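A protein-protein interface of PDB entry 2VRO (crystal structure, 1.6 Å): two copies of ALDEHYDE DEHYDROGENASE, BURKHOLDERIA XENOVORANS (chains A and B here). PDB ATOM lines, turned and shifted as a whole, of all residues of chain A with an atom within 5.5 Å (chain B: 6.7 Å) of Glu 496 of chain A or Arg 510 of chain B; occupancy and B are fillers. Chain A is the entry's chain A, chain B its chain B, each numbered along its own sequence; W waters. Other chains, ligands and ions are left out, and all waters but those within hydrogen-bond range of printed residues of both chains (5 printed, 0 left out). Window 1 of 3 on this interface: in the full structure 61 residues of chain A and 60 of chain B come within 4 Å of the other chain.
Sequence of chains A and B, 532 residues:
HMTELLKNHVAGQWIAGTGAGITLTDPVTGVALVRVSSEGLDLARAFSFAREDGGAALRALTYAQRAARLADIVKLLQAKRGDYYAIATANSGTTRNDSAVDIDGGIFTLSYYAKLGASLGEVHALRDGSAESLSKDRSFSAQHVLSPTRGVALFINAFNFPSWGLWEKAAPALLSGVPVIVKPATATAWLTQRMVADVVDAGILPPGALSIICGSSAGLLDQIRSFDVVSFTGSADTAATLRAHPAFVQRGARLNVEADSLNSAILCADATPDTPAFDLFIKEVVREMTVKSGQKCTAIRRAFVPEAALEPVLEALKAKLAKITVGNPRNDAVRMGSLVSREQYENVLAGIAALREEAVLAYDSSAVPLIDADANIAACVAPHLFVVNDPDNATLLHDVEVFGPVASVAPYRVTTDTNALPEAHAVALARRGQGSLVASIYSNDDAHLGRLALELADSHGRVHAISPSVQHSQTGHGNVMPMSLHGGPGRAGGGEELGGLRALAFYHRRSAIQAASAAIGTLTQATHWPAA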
ATOM      1  N   ASN A 256     -25.966 -24.693  11.951  1.00  0.00           N
ATOM      2  CA  ASN A 256     -25.632 -24.540  10.549  1.00  0.00           C
ATOM      3  C   ASN A 256     -24.356 -25.289  10.277  1.00  0.00           C
ATOM      4  O   ASN A 256     -23.378 -25.139  11.012  1.00  0.00           O
ATOM      5  CB  ASN A 256     -25.440 -23.067  10.201  1.00  0.00           C
ATOM      6  CG  ASN A 256     -25.411 -22.818   8.691  1.00  0.00           C
ATOM      7  OD1 ASN A 256     -24.338 -22.716   8.072  1.00  0.00           O
ATOM      8  ND2 ASN A 256     -26.589 -22.732   8.097  1.00  0.00           N
ATOM      9  N   VAL A 257     -24.371 -26.084   9.209  1.00  0.00           N
ATOM     10  CA  VAL A 257     -23.203 -26.846   8.798  1.00  0.00           C
ATOM     11  C   VAL A 257     -22.758 -26.425   7.402  1.00  0.00           C
ATOM     12  O   VAL A 257     -23.584 -26.332   6.491  1.00  0.00           O
ATOM     13  CB  VAL A 257     -23.508 -28.374   8.806  1.00  0.00           C
ATOM     14  CG1 VAL A 257     -22.371 -29.206   8.155  1.00  0.00           C
ATOM     15  CG2 VAL A 257     -23.784 -28.860  10.234  1.00  0.00           C
ATOM     16  N   ALA A 457     -29.160 -24.790 -10.195  1.00  0.00           N
ATOM     17  CA  ALA A 457     -29.534 -24.112  -8.951  1.00  0.00           C
ATOM     18  C   ALA A 457     -30.024 -25.043  -7.815  1.00  0.00           C
ATOM     19  O   ALA A 457     -29.760 -24.769  -6.637  1.00  0.00           O
ATOM     20  CB  ALA A 457     -30.543 -22.985  -9.235  1.00  0.00           C
ATOM     21  N   HIS A 460     -26.739 -26.634  -6.196  1.00  0.00           N
ATOM     22  CA  HIS A 460     -25.616 -25.763  -5.853  1.00  0.00           C
ATOM     23  C   HIS A 460     -26.089 -24.515  -5.136  1.00  0.00           C
ATOM     24  O   HIS A 460     -27.013 -23.842  -5.608  1.00  0.00           O
ATOM     25  CB  HIS A 460     -24.826 -25.370  -7.100  1.00  0.00           C
ATOM     26  CG  HIS A 460     -24.232 -26.543  -7.815  1.00  0.00           C
ATOM     27  ND1 HIS A 460     -24.962 -27.323  -8.688  1.00  0.00           N
ATOM     28  CD2 HIS A 460     -22.994 -27.090  -7.761  1.00  0.00           C
ATOM     29  CE1 HIS A 460     -24.196 -28.301  -9.145  1.00  0.00           C
ATOM     30  NE2 HIS A 460     -22.997 -28.178  -8.605  1.00  0.00           N
ATOM     31  N   GLY A 461     -25.443 -24.195  -4.015  1.00  0.00           N
ATOM     32  CA  GLY A 461     -25.784 -22.969  -3.246  1.00  0.00           C
ATOM     33  C   GLY A 461     -25.481 -21.695  -4.026  1.00  0.00           C
ATOM     34  O   GLY A 461     -26.102 -20.638  -3.820  1.00  0.00           O
ATOM     35  N   LEU A 485     -25.462 -15.503  -0.970  1.00  0.00           N
ATOM     36  CA  LEU A 485     -25.602 -16.683  -0.128  1.00  0.00           C
ATOM     37  C   LEU A 485     -24.401 -17.614  -0.236  1.00  0.00           C
ATOM     38  O   LEU A 485     -23.846 -17.814  -1.324  1.00  0.00           O
ATOM     39  CB  LEU A 485     -26.873 -17.437  -0.505  1.00  0.00           C
ATOM     40  CG  LEU A 485     -27.613 -18.183   0.606  1.00  0.00           C
ATOM     41  CD1 LEU A 485     -28.276 -17.167   1.584  1.00  0.00           C
ATOM     42  CD2 LEU A 485     -28.646 -19.137   0.009  1.00  0.00           C
ATOM     43  N   HIS A 486     -24.018 -18.168   0.914  1.00  0.00           N
ATOM     44  CA  HIS A 486     -22.939 -19.133   1.026  1.00  0.00           C
ATOM     45  C   HIS A 486     -23.420 -20.387   1.767  1.00  0.00           C
ATOM     46  O   HIS A 486     -23.919 -20.308   2.885  1.00  0.00           O
ATOM     47  CB  HIS A 486     -21.759 -18.516   1.776  1.00  0.00           C
ATOM     48  CG  HIS A 486     -20.629 -19.467   1.986  1.00  0.00           C
ATOM     49  ND1 HIS A 486     -20.002 -20.114   0.940  1.00  0.00           N
ATOM     50  CD2 HIS A 486     -20.022 -19.901   3.120  1.00  0.00           C
ATOM     51  CE1 HIS A 486     -19.049 -20.897   1.420  1.00  0.00           C
ATOM     52  NE2 HIS A 486     -19.057 -20.800   2.740  1.00  0.00           N
ATOM     53  N   GLY A 487     -23.228 -21.541   1.148  1.00  0.00           N
ATOM     54  CA  GLY A 487     -23.770 -22.793   1.673  1.00  0.00           C
ATOM     55  C   GLY A 487     -24.227 -23.613   0.496  1.00  0.00           C
ATOM     56  O   GLY A 487     -24.123 -23.177  -0.670  1.00  0.00           O
ATOM     57  N   GLY A 494     -26.319 -28.353   3.808  1.00  0.00           N
ATOM     58  CA  GLY A 494     -27.685 -27.819   3.868  1.00  0.00           C
ATOM     59  C   GLY A 494     -27.782 -26.477   4.592  1.00  0.00           C
ATOM     60  O   GLY A 494     -28.878 -26.026   4.950  1.00  0.00           O
ATOM     61  N   GLY A 495     -26.629 -25.841   4.785  1.00  0.00           N
ATOM     62  CA  GLY A 495     -26.515 -24.614   5.550  1.00  0.00           C
ATOM     63  C   GLY A 495     -26.701 -23.412   4.636  1.00  0.00           C
ATOM     64  O   GLY A 495     -26.655 -23.518   3.395  1.00  0.00           O
ATOM     65  N   GLU A 496     -26.902 -22.259   5.268  1.00  0.00           N
ATOM     66  CA  GLU A 496     -26.995 -20.994   4.578  1.00  0.00           C
ATOM     67  C   GLU A 496     -26.330 -19.962   5.470  1.00  0.00           C
ATOM     68  O   GLU A 496     -26.633 -19.879   6.659  1.00  0.00           O
ATOM     69  CB  GLU A 496     -28.453 -20.611   4.350  1.00  0.00           C
ATOM     70  CG  GLU A 496     -29.183 -21.545   3.399  1.00  0.00           C
ATOM     71  CD  GLU A 496     -30.409 -20.918   2.750  1.00  0.00           C
ATOM     72  OE1 GLU A 496     -30.816 -19.800   3.145  1.00  0.00           O
ATOM     73  OE2 GLU A 496     -30.962 -21.569   1.832  1.00  0.00           O
ATOM     74  N   GLU A 497     -25.406 -19.215   4.882  1.00  0.00           N
ATOM     75  CA  GLU A 497     -24.732 -18.120   5.546  1.00  0.00           C
ATOM     76  C   GLU A 497     -24.728 -16.914   4.607  1.00  0.00           C
ATOM     77  O   GLU A 497     -24.964 -17.056   3.411  1.00  0.00           O
ATOM     78  CB  GLU A 497     -23.276 -18.467   5.837  1.00  0.00           C
ATOM     79  CG  GLU A 497     -23.041 -19.555   6.847  1.00  0.00           C
ATOM     80  CD  GLU A 497     -21.552 -19.709   7.149  1.00  0.00           C
ATOM     81  OE1 GLU A 497     -20.764 -20.117   6.259  1.00  0.00           O
ATOM     82  OE2 GLU A 497     -21.168 -19.404   8.276  1.00  0.00           O
ATOM     83  N   LEU A 498     -24.438 -15.746   5.167  1.00  0.00           N
ATOM     84  CA  LEU A 498     -24.234 -14.525   4.383  1.00  0.00           C
ATOM     85  C   LEU A 498     -25.482 -14.193   3.544  1.00  0.00           C
ATOM     86  O   LEU A 498     -26.597 -14.305   4.047  1.00  0.00           O
ATOM     87  CB  LEU A 498     -22.928 -14.603   3.563  1.00  0.00           C
ATOM     88  CG  LEU A 498     -21.631 -14.687   4.401  1.00  0.00           C
ATOM     89  CD1 LEU A 498     -20.449 -15.060   3.519  1.00  0.00           C
ATOM     90  CD2 LEU A 498     -21.351 -13.400   5.164  1.00  0.00           C
ATOM     91  N   ARG A 502     -29.925 -11.660   4.646  1.00  0.00           N
ATOM     92  CA  ARG A 502     -30.407 -13.030   4.797  1.00  0.00           C
ATOM     93  C   ARG A 502     -29.746 -13.713   5.992  1.00  0.00           C
ATOM     94  O   ARG A 502     -30.373 -14.513   6.682  1.00  0.00           O
ATOM     95  CB  ARG A 502     -30.176 -13.835   3.521  1.00  0.00           C
ATOM     96  CG  ARG A 502     -31.029 -13.355   2.348  1.00  0.00           C
ATOM     97  CD  ARG A 502     -30.656 -14.111   1.082  1.00  0.00           C
ATOM     98  NE  ARG A 502     -31.356 -13.569  -0.087  1.00  0.00           N
ATOM     99  CZ  ARG A 502     -31.000 -12.454  -0.726  1.00  0.00           C
ATOM    100  NH1 ARG A 502     -29.955 -11.729  -0.310  1.00  0.00           N
ATOM    101  NH2 ARG A 502     -31.705 -12.062  -1.789  1.00  0.00           N
ATOM    102  N   ASP B 128     -35.897 -14.603  -5.486  1.00  0.00           N
ATOM    103  CA  ASP B 128     -35.662 -14.206  -4.102  1.00  0.00           C
ATOM    104  C   ASP B 128     -34.974 -12.838  -4.018  1.00  0.00           C
ATOM    105  O   ASP B 128     -33.780 -12.732  -4.269  1.00  0.00           O
ATOM    106  CB  ASP B 128     -34.815 -15.248  -3.377  1.00  0.00           C
ATOM    107  CG  ASP B 128     -34.507 -14.836  -1.941  1.00  0.00           C
ATOM    108  OD1 ASP B 128     -33.458 -14.214  -1.705  1.00  0.00           O
ATOM    109  OD2 ASP B 128     -35.318 -15.119  -1.048  1.00  0.00           O
ATOM    110  N   HIS B 144     -30.569 -14.043  -6.447  1.00  0.00           N
ATOM    111  CA  HIS B 144     -30.937 -15.280  -5.762  1.00  0.00           C
ATOM    112  C   HIS B 144     -32.227 -15.841  -6.331  1.00  0.00           C
ATOM    113  O   HIS B 144     -33.145 -15.084  -6.696  1.00  0.00           O
ATOM    114  CB  HIS B 144     -31.085 -15.030  -4.257  1.00  0.00           C
ATOM    115  CG  HIS B 144     -29.797 -14.663  -3.589  1.00  0.00           C
ATOM    116  ND1 HIS B 144     -29.269 -13.389  -3.631  1.00  0.00           N
ATOM    117  CD2 HIS B 144     -28.911 -15.410  -2.891  1.00  0.00           C
ATOM    118  CE1 HIS B 144     -28.130 -13.361  -2.965  1.00  0.00           C
ATOM    119  NE2 HIS B 144     -27.892 -14.575  -2.500  1.00  0.00           N
ATOM    120  N   VAL B 145     -32.302 -17.171  -6.371  1.00  0.00           N
ATOM    121  CA  VAL B 145     -33.517 -17.877  -6.776  1.00  0.00           C
ATOM    122  C   VAL B 145     -33.873 -19.011  -5.816  1.00  0.00           C
ATOM    123  O   VAL B 145     -33.009 -19.499  -5.067  1.00  0.00           O
ATOM    124  CB  VAL B 145     -33.419 -18.464  -8.216  1.00  0.00           C
ATOM    125  CG1 VAL B 145     -33.208 -17.368  -9.245  1.00  0.00           C
ATOM    126  CG2 VAL B 145     -32.305 -19.511  -8.328  1.00  0.00           C
ATOM    127  N   LEU B 146     -35.151 -19.400  -5.857  1.00  0.00           N
ATOM    128  CA  LEU B 146     -35.661 -20.593  -5.189  1.00  0.00           C
ATOM    129  C   LEU B 146     -36.047 -21.637  -6.225  1.00  0.00           C
ATOM    130  O   LEU B 146     -36.800 -21.342  -7.161  1.00  0.00           O
ATOM    131  CB  LEU B 146     -36.906 -20.271  -4.347  1.00  0.00           C
ATOM    132  CG  LEU B 146     -36.837 -19.233  -3.223  1.00  0.00           C
ATOM    133  CD1 LEU B 146     -38.168 -19.275  -2.458  1.00  0.00           C
ATOM    134  CD2 LEU B 146     -35.684 -19.497  -2.279  1.00  0.00           C
ATOM    135  N   SER B 147     -35.545 -22.853  -6.030  1.00  0.00           N
ATOM    136  CA  SER B 147     -35.854 -24.000  -6.897  1.00  0.00           C
ATOM    137  C   SER B 147     -36.431 -25.105  -6.024  1.00  0.00           C
ATOM    138  O   SER B 147     -35.933 -25.326  -4.922  1.00  0.00           O
ATOM    139  CB  SER B 147     -34.595 -24.527  -7.582  1.00  0.00           C
ATOM    140  OG  SER B 147     -33.896 -23.492  -8.242  1.00  0.00           O
ATOM    141  N   ARG B 254     -34.171 -32.071   5.847  1.00  0.00           N
ATOM    142  CA  ARG B 254     -34.793 -31.021   6.660  1.00  0.00           C
ATOM    143  C   ARG B 254     -35.893 -31.588   7.541  1.00  0.00           C
ATOM    144  O   ARG B 254     -36.671 -32.461   7.128  1.00  0.00           O
ATOM    145  CB  ARG B 254     -35.362 -29.892   5.793  1.00  0.00           C
ATOM    146  CG  ARG B 254     -34.331 -29.185   4.953  1.00  0.00           C
ATOM    147  CD  ARG B 254     -34.976 -27.996   4.221  1.00  0.00           C
ATOM    148  NE  ARG B 254     -33.950 -27.171   3.583  1.00  0.00           N
ATOM    149  CZ  ARG B 254     -34.194 -26.262   2.640  1.00  0.00           C
ATOM    150  NH1 ARG B 254     -35.430 -26.058   2.221  1.00  0.00           N
ATOM    151  NH2 ARG B 254     -33.198 -25.564   2.120  1.00  0.00           N
ATOM    152  N   ALA B 505     -40.126 -21.531   1.479  1.00  0.00           N
ATOM    153  CA  ALA B 505     -38.671 -21.723   1.632  1.00  0.00           C
ATOM    154  C   ALA B 505     -38.349 -23.169   2.010  1.00  0.00           C
ATOM    155  O   ALA B 505     -37.380 -23.754   1.512  1.00  0.00           O
ATOM    156  CB  ALA B 505     -38.099 -20.756   2.692  1.00  0.00           C
ATOM    157  N   HIS B 508     -37.943 -25.406  -0.955  1.00  0.00           N
ATOM    158  CA  HIS B 508     -37.022 -24.961  -2.000  1.00  0.00           C
ATOM    159  C   HIS B 508     -35.562 -24.977  -1.539  1.00  0.00           C
ATOM    160  O   HIS B 508     -35.276 -25.061  -0.336  1.00  0.00           O
ATOM    161  CB  HIS B 508     -37.398 -23.536  -2.449  1.00  0.00           C
ATOM    162  CG  HIS B 508     -38.677 -23.449  -3.235  1.00  0.00           C
ATOM    163  ND1 HIS B 508     -39.925 -23.511  -2.649  1.00  0.00           N
ATOM    164  CD2 HIS B 508     -38.897 -23.300  -4.566  1.00  0.00           C
ATOM    165  CE1 HIS B 508     -40.856 -23.382  -3.578  1.00  0.00           C
ATOM    166  NE2 HIS B 508     -40.259 -23.247  -4.751  1.00  0.00           N
ATOM    167  N   ARG B 509     -34.634 -24.926  -2.490  1.00  0.00           N
ATOM    168  CA  ARG B 509     -33.257 -24.533  -2.170  1.00  0.00           C
ATOM    169  C   ARG B 509     -33.046 -23.137  -2.731  1.00  0.00           C
ATOM    170  O   ARG B 509     -33.452 -22.844  -3.861  1.00  0.00           O
ATOM    171  CB  ARG B 509     -32.182 -25.502  -2.707  1.00  0.00           C
ATOM    172  CG  ARG B 509     -30.702 -25.006  -2.494  1.00  0.00           C
ATOM    173  CD  ARG B 509     -30.177 -25.029  -1.026  1.00  0.00           C
ATOM    174  NE  ARG B 509     -29.281 -23.895  -0.703  1.00  0.00           N
ATOM    175  CZ  ARG B 509     -28.519 -23.792   0.393  1.00  0.00           C
ATOM    176  NH1 ARG B 509     -28.481 -24.760   1.305  1.00  0.00           N
ATOM    177  NH2 ARG B 509     -27.756 -22.709   0.574  1.00  0.00           N
ATOM    178  N   ARG B 510     -32.451 -22.280  -1.919  1.00  0.00           N
ATOM    179  CA  ARG B 510     -32.101 -20.939  -2.340  1.00  0.00           C
ATOM    180  C   ARG B 510     -30.702 -20.966  -2.912  1.00  0.00           C
ATOM    181  O   ARG B 510     -29.783 -21.502  -2.281  1.00  0.00           O
ATOM    182  CB  ARG B 510     -32.150 -19.998  -1.142  1.00  0.00           C
ATOM    183  CG  ARG B 510     -31.853 -18.535  -1.445  1.00  0.00           C
ATOM    184  CD  ARG B 510     -32.056 -17.696  -0.166  1.00  0.00           C
ATOM    185  NE  ARG B 510     -33.459 -17.672   0.240  1.00  0.00           N
ATOM    186  CZ  ARG B 510     -33.990 -18.427   1.206  1.00  0.00           C
ATOM    187  NH1 ARG B 510     -33.228 -19.268   1.903  1.00  0.00           N
ATOM    188  NH2 ARG B 510     -35.286 -18.333   1.487  1.00  0.00           N
ATOM    189  N   SER B 511     -30.521 -20.361  -4.084  1.00  0.00           N
ATOM    190  CA  SER B 511     -29.192 -20.280  -4.669  1.00  0.00           C
ATOM    191  C   SER B 511     -28.875 -18.880  -5.135  1.00  0.00           C
ATOM    192  O   SER B 511     -29.768 -18.168  -5.624  1.00  0.00           O
ATOM    193  CB  SER B 511     -29.073 -21.257  -5.835  1.00  0.00           C
ATOM    194  OG  SER B 511     -29.388 -22.556  -5.357  1.00  0.00           O
ATOM    195  N   ALA B 512     -27.610 -18.492  -4.964  1.00  0.00           N
ATOM    196  CA  ALA B 512     -27.090 -17.236  -5.519  1.00  0.00           C
ATOM    197  C   ALA B 512     -26.545 -17.483  -6.927  1.00  0.00           C
ATOM    198  O   ALA B 512     -25.691 -18.364  -7.128  1.00  0.00           O
ATOM    199  CB  ALA B 512     -25.983 -16.662  -4.631  1.00  0.00           C
HETATM  200  O   HOH W   1     -32.582 -23.136   0.762  1.00  0.00           O
HETATM  201  O   HOH W   2     -32.426 -16.769   2.961  1.00  0.00           O
HETATM  202  O   HOH W   3     -31.291 -27.794   4.139  1.00  0.00           O
HETATM  203  O   HOH W   4     -32.098 -22.698  -6.285  1.00  0.00           O
HETATM  204  O   HOH W   5     -31.309 -11.587  -4.936  1.00  0.00           O
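O of Ala 457 of chain A lies within hydrogen-bond range of OG of Ser 511 of chain B, at 2.6 Å. O of His 460 of chain A sits at hydrogen-bond distance from OG of Ser 511 of chain B (2.7 Å). The backbone carbonyl oxygen (O) of Gly 461 of chain A lies within hydrogen-bond range of the backbone NH (N) of Ala 512 of chain B (2.9 Å). NE2 of His 144 of chain B is in hydrogen-bond range of N of Leu 485 of chain A, at 3.0 Å. The guanidinium group (NH1) of Arg 509 of chain B lies within hydrogen-bond range of the backbone carbonyl oxygen (O) of Gly 495 of chain A (3.0 Å). The guanidinium group of Arg 509 of chain B lies within salt-bridge range of the side-chain carboxylate of Glu 496 of chain A, at 3.6 Å. NH1 of Arg 510 of chain B lies within salt-bridge range of OE1 of Glu 496 of chain A, 2.8 Å away. The side-chain carboxylate (OD1) of Asp 128 of chain B lies within salt-bridge range of the guanidinium group (NE) of Arg 502 of chain A, 2.7 Å away. A ring nitrogen (ND1) of His 144 of chain B lies within hydrogen-bond range of the guanidinium group of Arg 502 of chain A, at 3.3 Å.
The side-chain amide nitrogen of Asn 256 of chain A sits close to the backbone NH of Glu 496 of chain A (2.9 Å). The backbone NH (N) of Asp 128 of chain B lies within hydrogen-bond range of the backbone carbonyl oxygen (O) of His 144 of chain B, 3.0 Å away. The side-chain carboxylate (OD2) of Asp 128 of chain B lies within salt-bridge range of the guanidinium group (NE) of Arg 510 of chain B. The backbone carbonyl oxygen (O) of Val 145 of chain B sits at hydrogen-bond distance from the backbone NH (N) of Ser 511 of chain B, 2.8 Å away. The backbone carbonyl oxygen of Ser 147 of chain B is in hydrogen-bond range of the backbone NH of Arg 509 of chain B (2.8 Å).
Ala 457 of chain A touches Val 145 of chain B (CB to CG2, 3.999 Å). Ala 457 of chain A touches Ser 147 of chain B (CB to OG, 3.5 Å). CA of Ser 511 of chain B touches O of Gly 461 of chain A, at 3.2 Å. CD2 of Leu 485 of chain A touches NH2 of Arg 509 of chain B, at 3.7 Å. O of Arg 510 of chain B touches CD2 of Leu 485 of chain A, 3.5 Å away. Leu 485 of chain A touches Ala 512 of chain B. Arg 509 of chain B touches Gly 487 of chain A. Gly 494 of chain A touches Arg 509 of chain B.
Of the printed residues of chain B, His 460 of chain A touches Ser 511. Of the printed residues of chain B, Gly 487 of chain A touches Arg 509 (3.6 Å). Ala 505 of chain B touches none of the printed residues of chain A. His 508 of chain B touches none of the printed residues of chain A.
Along chain A the printed residues that touch a printed residue of chain B span positions 457 to 502. Among the printed residues, 17 pairs touch across the chains. Among the printed residues, Asp or Glu carboxylates within 4 Å of a Lys or Arg side-chain nitrogen of the other chain: Glu 496 of chain A with Arg 509 of chain B (3.6 Å), Glu 496 of chain A with Arg 510 of chain B (2.8 Å) and Arg 502 of chain A with Asp 128 of chain B (2.7 Å).
No position is printed for both chains. Of the 17 pairs that touch across the chains among the printed residues, none has its exchanged pair printed and touching as well.
Water W1 lies within hydrogen-bond range of OE2 of Glu 496 of chain A (2.5 Å), N of Arg 510 of chain B (2.8 Å), NH2 of Arg 254 of chain B (2.8 Å) and O of His 508 of chain B (3.5 Å). Water W4 lies within hydrogen-bond range of the side-chain hydroxyl (OG) of Ser 147 of chain B (2.8 Å), the backbone carbonyl oxygen (O) of Arg 509 of chain B (2.8 Å), the side-chain hydroxyl (OG) of Ser 511 of chain B (2.9 Å) and the backbone carbonyl oxygen (O) of Ala 457 of chain A (3.1 Å). Water W3 bridges the guanidinium group of Arg 254 of chain B and the backbone carbonyl oxygen of Gly 494 of chain A. Water W5 lies within hydrogen-bond range of the backbone carbonyl oxygen of Asp 128 of chain B (2.8 Å), the backbone NH of His 144 of chain B (3.0 Å) and the guanidinium group of Arg 502 of chain A (3.2 Å). Water W2 lies within hydrogen-bond range of the guanidinium group of Arg 510 of chain B and the side-chain carboxylate of Glu 496 of chain A.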
